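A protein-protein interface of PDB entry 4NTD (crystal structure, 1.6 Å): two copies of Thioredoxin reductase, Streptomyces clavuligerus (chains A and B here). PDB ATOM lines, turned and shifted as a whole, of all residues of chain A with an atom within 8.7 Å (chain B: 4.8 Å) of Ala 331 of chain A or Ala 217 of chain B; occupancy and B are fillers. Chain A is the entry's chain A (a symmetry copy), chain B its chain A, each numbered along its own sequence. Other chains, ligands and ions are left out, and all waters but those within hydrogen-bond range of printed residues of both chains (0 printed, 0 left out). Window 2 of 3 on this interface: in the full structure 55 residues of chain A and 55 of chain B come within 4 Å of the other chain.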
ATOM      1  N   VAL A 324      -0.407   2.791  11.375  1.00  0.00           N
ATOM      2  CA  VAL A 324       0.877   3.461  11.597  1.00  0.00           C
ATOM      3  C   VAL A 324       1.677   2.717  12.670  1.00  0.00           C
ATOM      4  O   VAL A 324       2.867   2.467  12.489  1.00  0.00           O
ATOM      5  CB  VAL A 324       0.704   4.946  11.988  1.00  0.00           C
ATOM      6  CG1 VAL A 324       2.030   5.546  12.446  1.00  0.00           C
ATOM      7  CG2 VAL A 324       0.147   5.741  10.816  1.00  0.00           C
ATOM      8  N   ASP A 325       1.023   2.349  13.770  1.00  0.00           N
ATOM      9  CA  ASP A 325       1.692   1.583  14.827  1.00  0.00           C
ATOM     10  C   ASP A 325       2.298   0.290  14.269  1.00  0.00           C
ATOM     11  O   ASP A 325       3.422  -0.070  14.618  1.00  0.00           O
ATOM     12  CB  ASP A 325       0.731   1.265  15.980  1.00  0.00           C
ATOM     13  CG  ASP A 325       0.313   2.502  16.765  1.00  0.00           C
ATOM     14  OD1 ASP A 325      -0.685   2.416  17.509  1.00  0.00           O
ATOM     15  OD2 ASP A 325       0.971   3.557  16.649  1.00  0.00           O
ATOM     16  N   GLU A 326       1.562  -0.393  13.395  1.00  0.00           N
ATOM     17  CA  GLU A 326       2.081  -1.598  12.741  1.00  0.00           C
ATOM     18  C   GLU A 326       3.214  -1.270  11.761  1.00  0.00           C
ATOM     19  O   GLU A 326       4.223  -1.977  11.727  1.00  0.00           O
ATOM     20  CB  GLU A 326       0.967  -2.361  12.019  1.00  0.00           C
ATOM     21  CG  GLU A 326       1.399  -3.743  11.545  1.00  0.00           C
ATOM     22  CD  GLU A 326       0.341  -4.444  10.721  1.00  0.00           C
ATOM     23  OE1 GLU A 326      -0.788  -4.627  11.221  1.00  0.00           O
ATOM     24  OE2 GLU A 326       0.645  -4.818   9.571  1.00  0.00           O
ATOM     25  N   ASP A 327       3.042  -0.208  10.969  1.00  0.00           N
ATOM     26  CA  ASP A 327       4.079   0.246  10.031  1.00  0.00           C
ATOM     27  C   ASP A 327       5.396   0.522  10.774  1.00  0.00           C
ATOM     28  O   ASP A 327       6.472   0.124  10.318  1.00  0.00           O
ATOM     29  CB  ASP A 327       3.638   1.517   9.277  1.00  0.00           C
ATOM     30  CG  ASP A 327       2.497   1.270   8.283  1.00  0.00           C
ATOM     31  OD1 ASP A 327       2.342   0.132   7.790  1.00  0.00           O
ATOM     32  OD2 ASP A 327       1.754   2.236   7.988  1.00  0.00           O
ATOM     33  N   VAL A 328       5.300   1.188  11.924  1.00  0.00           N
ATOM     34  CA  VAL A 328       6.474   1.527  12.734  1.00  0.00           C
ATOM     35  C   VAL A 328       7.115   0.274  13.334  1.00  0.00           C
ATOM     36  O   VAL A 328       8.329   0.095  13.248  1.00  0.00           O
ATOM     37  CB  VAL A 328       6.121   2.525  13.862  1.00  0.00           C
ATOM     38  CG1 VAL A 328       7.298   2.727  14.813  1.00  0.00           C
ATOM     39  CG2 VAL A 328       5.696   3.864  13.276  1.00  0.00           C
ATOM     40  N   ALA A 329       6.295  -0.585  13.938  1.00  0.00           N
ATOM     41  CA  ALA A 329       6.790  -1.820  14.556  1.00  0.00           C
ATOM     42  C   ALA A 329       7.489  -2.726  13.539  1.00  0.00           C
ATOM     43  O   ALA A 329       8.520  -3.327  13.846  1.00  0.00           O
ATOM     44  CB  ALA A 329       5.655  -2.565  15.243  1.00  0.00           C
ATOM     45  N   SER A 330       6.934  -2.810  12.332  1.00  0.00           N
ATOM     46  CA  SER A 330       7.534  -3.601  11.255  1.00  0.00           C
ATOM     47  C   SER A 330       8.860  -3.011  10.767  1.00  0.00           C
ATOM     48  O   SER A 330       9.795  -3.752  10.456  1.00  0.00           O
ATOM     49  CB  SER A 330       6.563  -3.739  10.080  1.00  0.00           C
ATOM     50  OG  SER A 330       5.425  -4.499  10.449  1.00  0.00           O
ATOM     51  N   ALA A 331       8.936  -1.683  10.697  1.00  0.00           N
ATOM     52  CA  ALA A 331      10.166  -0.996  10.295  1.00  0.00           C
ATOM     53  C   ALA A 331      11.264  -1.156  11.347  1.00  0.00           C
ATOM     54  O   ALA A 331      12.430  -1.359  11.006  1.00  0.00           O
ATOM     55  CB  ALA A 331       9.894   0.479  10.036  1.00  0.00           C
ATOM     56  N   VAL A 332      10.887  -1.059  12.620  1.00  0.00           N
ATOM     57  CA  VAL A 332      11.827  -1.256  13.730  1.00  0.00           C
ATOM     58  C   VAL A 332      12.363  -2.693  13.725  1.00  0.00           C
ATOM     59  O   VAL A 332      13.564  -2.915  13.895  1.00  0.00           O
ATOM     60  CB  VAL A 332      11.167  -0.925  15.092  1.00  0.00           C
ATOM     61  CG1 VAL A 332      12.015  -1.418  16.259  1.00  0.00           C
ATOM     62  CG2 VAL A 332      10.929   0.575  15.214  1.00  0.00           C
ATOM     63  N   ARG A 333      11.458  -3.648  13.525  1.00  0.00           N
ATOM     64  CA  ARG A 333      11.793  -5.072  13.412  1.00  0.00           C
ATOM     65  C   ARG A 333      12.805  -5.316  12.290  1.00  0.00           C
ATOM     66  O   ARG A 333      13.802  -6.017  12.471  1.00  0.00           O
ATOM     67  CB  ARG A 333      10.500  -5.875  13.165  1.00  0.00           C
ATOM     68  CG  ARG A 333      10.638  -7.185  12.396  1.00  0.00           C
ATOM     69  CD  ARG A 333       9.459  -7.376  11.449  1.00  0.00           C
ATOM     70  NE  ARG A 333       9.558  -6.509  10.273  1.00  0.00           N
ATOM     71  CZ  ARG A 333       8.774  -6.599   9.204  1.00  0.00           C
ATOM     72  NH1 ARG A 333       7.821  -7.520   9.151  1.00  0.00           N
ATOM     73  NH2 ARG A 333       8.945  -5.771   8.180  1.00  0.00           N
ATOM     74  N   ALA A 334      12.525  -4.741  11.123  1.00  0.00           N
ATOM     75  CA  ALA A 334      13.367  -4.933   9.935  1.00  0.00           C
ATOM     76  C   ALA A 334      14.748  -4.293  10.076  1.00  0.00           C
ATOM     77  O   ALA A 334      15.752  -4.884   9.671  1.00  0.00           O
ATOM     78  CB  ALA A 334      12.667  -4.393   8.696  1.00  0.00           C
ATOM     79  N   ALA A 335      14.793  -3.090  10.643  1.00  0.00           N
ATOM     80  CA  ALA A 335      16.058  -2.388  10.869  1.00  0.00           C
ATOM     81  C   ALA A 335      16.939  -3.127  11.876  1.00  0.00           C
ATOM     82  O   ALA A 335      18.163  -3.095  11.768  1.00  0.00           O
ATOM     83  CB  ALA A 335      15.799  -0.965  11.340  1.00  0.00           C
ATOM     84  N   ALA A 336      16.314  -3.785  12.850  1.00  0.00           N
ATOM     85  CA  ALA A 336      17.037  -4.574  13.851  1.00  0.00           C
ATOM     86  C   ALA A 336      17.507  -5.932  13.308  1.00  0.00           C
ATOM     87  O   ALA A 336      18.437  -6.527  13.850  1.00  0.00           O
ATOM     88  CB  ALA A 336      16.174  -4.771  15.089  1.00  0.00           C
ATOM     89  N   ARG A 337      16.856  -6.415  12.250  1.00  0.00           N
ATOM     90  CA  ARG A 337      17.252  -7.661  11.582  1.00  0.00           C
ATOM     91  C   ARG A 337      18.506  -7.457  10.744  1.00  0.00           C
ATOM     92  O   ARG A 337      19.516  -8.133  10.943  1.00  0.00           O
ATOM     93  CB  ARG A 337      16.127  -8.172  10.677  1.00  0.00           C
ATOM     94  CG  ARG A 337      15.318  -9.327  11.245  1.00  0.00           C
ATOM     95  CD  ARG A 337      13.915  -9.352  10.657  1.00  0.00           C
ATOM     96  NE  ARG A 337      13.892  -8.925   9.255  1.00  0.00           N
ATOM     97  CZ  ARG A 337      12.815  -8.469   8.615  1.00  0.00           C
ATOM     98  NH1 ARG A 337      11.640  -8.383   9.229  1.00  0.00           N
ATOM     99  NH2 ARG A 337      12.912  -8.097   7.343  1.00  0.00           N
ATOM    100  N   THR A 338      18.420  -6.525   9.796  1.00  0.00           N
ATOM    101  CA  THR A 338      19.558  -6.162   8.956  1.00  0.00           C
ATOM    102  C   THR A 338      20.652  -5.530   9.815  1.00  0.00           C
ATOM    103  O   THR A 338      21.840  -5.714   9.550  1.00  0.00           O
ATOM    104  CB  THR A 338      19.154  -5.174   7.841  1.00  0.00           C
ATOM    105  OG1 THR A 338      18.638  -3.970   8.424  1.00  0.00           O
ATOM    106  CG2 THR A 338      18.096  -5.784   6.921  1.00  0.00           C
ATOM    107  N   VAL A 339      20.221  -4.800  10.847  1.00  0.00           N
ATOM    108  CA  VAL A 339      21.097  -4.073  11.777  1.00  0.00           C
ATOM    109  C   VAL A 339      22.280  -3.425  11.044  1.00  0.00           C
ATOM    110  O   VAL A 339      23.401  -3.934  11.032  1.00  0.00           O
ATOM    111  CB  VAL A 339      21.478  -4.937  13.018  1.00  0.00           C
ATOM    112  CG1 VAL A 339      22.764  -5.741  12.831  1.00  0.00           C
ATOM    113  CG2 VAL A 339      21.573  -4.056  14.260  1.00  0.00           C
ATOM    114  N   ARG B 213      14.684   4.689  18.281  1.00  0.00           N
ATOM    115  CA  ARG B 213      14.620   3.546  17.359  1.00  0.00           C
ATOM    116  C   ARG B 213      13.496   3.704  16.328  1.00  0.00           C
ATOM    117  O   ARG B 213      13.686   3.419  15.144  1.00  0.00           O
ATOM    118  CB  ARG B 213      14.451   2.223  18.119  1.00  0.00           C
ATOM    119  CG  ARG B 213      15.746   1.656  18.679  1.00  0.00           C
ATOM    120  CD  ARG B 213      15.556   0.244  19.215  1.00  0.00           C
ATOM    121  NE  ARG B 213      14.834   0.229  20.487  1.00  0.00           N
ATOM    122  CZ  ARG B 213      15.390   0.392  21.689  1.00  0.00           C
ATOM    123  NH1 ARG B 213      16.699   0.589  21.822  1.00  0.00           N
ATOM    124  NH2 ARG B 213      14.625   0.358  22.775  1.00  0.00           N
ATOM    125  N   ALA B 214      12.334   4.169  16.779  1.00  0.00           N
ATOM    126  CA  ALA B 214      11.175   4.348  15.899  1.00  0.00           C
ATOM    127  C   ALA B 214      11.413   5.448  14.865  1.00  0.00           C
ATOM    128  O   ALA B 214      11.132   5.267  13.681  1.00  0.00           O
ATOM    129  CB  ALA B 214       9.932   4.656  16.719  1.00  0.00           C
ATOM    130  N   LEU B 215      11.934   6.584  15.323  1.00  0.00           N
ATOM    131  CA  LEU B 215      12.233   7.709  14.437  1.00  0.00           C
ATOM    132  C   LEU B 215      13.295   7.340  13.395  1.00  0.00           C
ATOM    133  O   LEU B 215      13.166   7.693  12.224  1.00  0.00           O
ATOM    134  CB  LEU B 215      12.665   8.933  15.253  1.00  0.00           C
ATOM    135  CG  LEU B 215      11.570   9.570  16.116  1.00  0.00           C
ATOM    136  CD1 LEU B 215      12.170  10.449  17.205  1.00  0.00           C
ATOM    137  CD2 LEU B 215      10.591  10.364  15.264  1.00  0.00           C
ATOM    138  N   SER B 216      14.333   6.618  13.820  1.00  0.00           N
ATOM    139  CA  SER B 216      15.353   6.118  12.891  1.00  0.00           C
ATOM    140  C   SER B 216      14.761   5.154  11.862  1.00  0.00           C
ATOM    141  O   SER B 216      15.042   5.263  10.666  1.00  0.00           O
ATOM    142  CB  SER B 216      16.490   5.423  13.650  1.00  0.00           C
ATOM    143  OG  SER B 216      17.251   6.357  14.391  1.00  0.00           O
ATOM    144  N   ALA B 217      13.932   4.225  12.331  1.00  0.00           N
ATOM    145  CA  ALA B 217      13.337   3.203  11.467  1.00  0.00           C
ATOM    146  C   ALA B 217      12.392   3.787  10.414  1.00  0.00           C
ATOM    147  O   ALA B 217      12.303   3.262   9.305  1.00  0.00           O
ATOM    148  CB  ALA B 217      12.611   2.161  12.305  1.00  0.00           C
ATOM    149  N   ARG B 218      11.691   4.866  10.761  1.00  0.00           N
ATOM    150  CA  ARG B 218      10.812   5.552   9.804  1.00  0.00           C
ATOM    151  C   ARG B 218      11.494   6.742   9.126  1.00  0.00           C
ATOM    152  O   ARG B 218      10.849   7.508   8.410  1.00  0.00           O
ATOM    153  CB  ARG B 218       9.506   5.988  10.480  1.00  0.00           C
ATOM    154  CG  ARG B 218       8.584   4.840  10.867  1.00  0.00           C
ATOM    155  CD  ARG B 218       8.087   4.059   9.655  1.00  0.00           C
ATOM    156  NE  ARG B 218       7.066   4.783   8.894  1.00  0.00           N
ATOM    157  CZ  ARG B 218       6.934   4.773   7.565  1.00  0.00           C
ATOM    158  NH1 ARG B 218       7.778   4.098   6.785  1.00  0.00           N
ATOM    159  NH2 ARG B 218       5.950   5.467   7.003  1.00  0.00           N
ATOM    160  N   GLN B 219      12.798   6.883   9.353  1.00  0.00           N
ATOM    161  CA  GLN B 219      13.627   7.860   8.652  1.00  0.00           C
ATOM    162  C   GLN B 219      13.108   9.294   8.826  1.00  0.00           C
ATOM    163  O   GLN B 219      12.907  10.031   7.859  1.00  0.00           O
ATOM    164  CB  GLN B 219      13.809   7.436   7.186  1.00  0.00           C
ATOM    165  CG  GLN B 219      14.470   6.061   7.093  1.00  0.00           C
ATOM    166  CD  GLN B 219      14.736   5.578   5.677  1.00  0.00           C
ATOM    167  OE1 GLN B 219      13.909   5.751   4.783  1.00  0.00           O
ATOM    168  NE2 GLN B 219      15.890   4.939   5.474  1.00  0.00           N
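CB of Ala 214 of chain B touches CG1 of Val 328 of chain A (3.8 Å).
Arg 218 of chain B touches Val 328 of chain A (CG to CG2, 3.9 Å).
Ala 331 of chain A touches Ala 217 of chain B (C to CB, 3.7 Å).
CG2 of Val 332 of chain A touches O of Arg 213 of chain B (3.96 Å).
Val 332 of chain A touches Ala 214 of chain B.
N of Val 332 of chain A touches CB of Ala 217 of chain B, at 3.7 Å.
Hydrophobic or aromatic side chains of chain A within 4 Å of the printed part of chain B: Val 328, Ala 331 and Val 332.
Among the printed residues, 6 pairs touch across the chains.
No position is printed for both chains.
Of chain A, only Ala 331 and Val 332 come within 4 Å of Ala 217 of chain B.
No residue of chain A comes within 4 Å of Ser 216 of chain B.
Printed residues of chain B within 4 Å of Val 328 of chain A: Ala 214 (3.8 Å) and Arg 218 (3.9 Å).
Of the printed residues of chain B, Val 332 of chain A touches Arg 213 (3.96 Å), Ala 214 (3.8 Å) and Ala 217 (3.7 Å).
The nearest printed residue of chain B that does not touch Val 332 of chain A is Leu 215 of chain B (6.1 Å).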
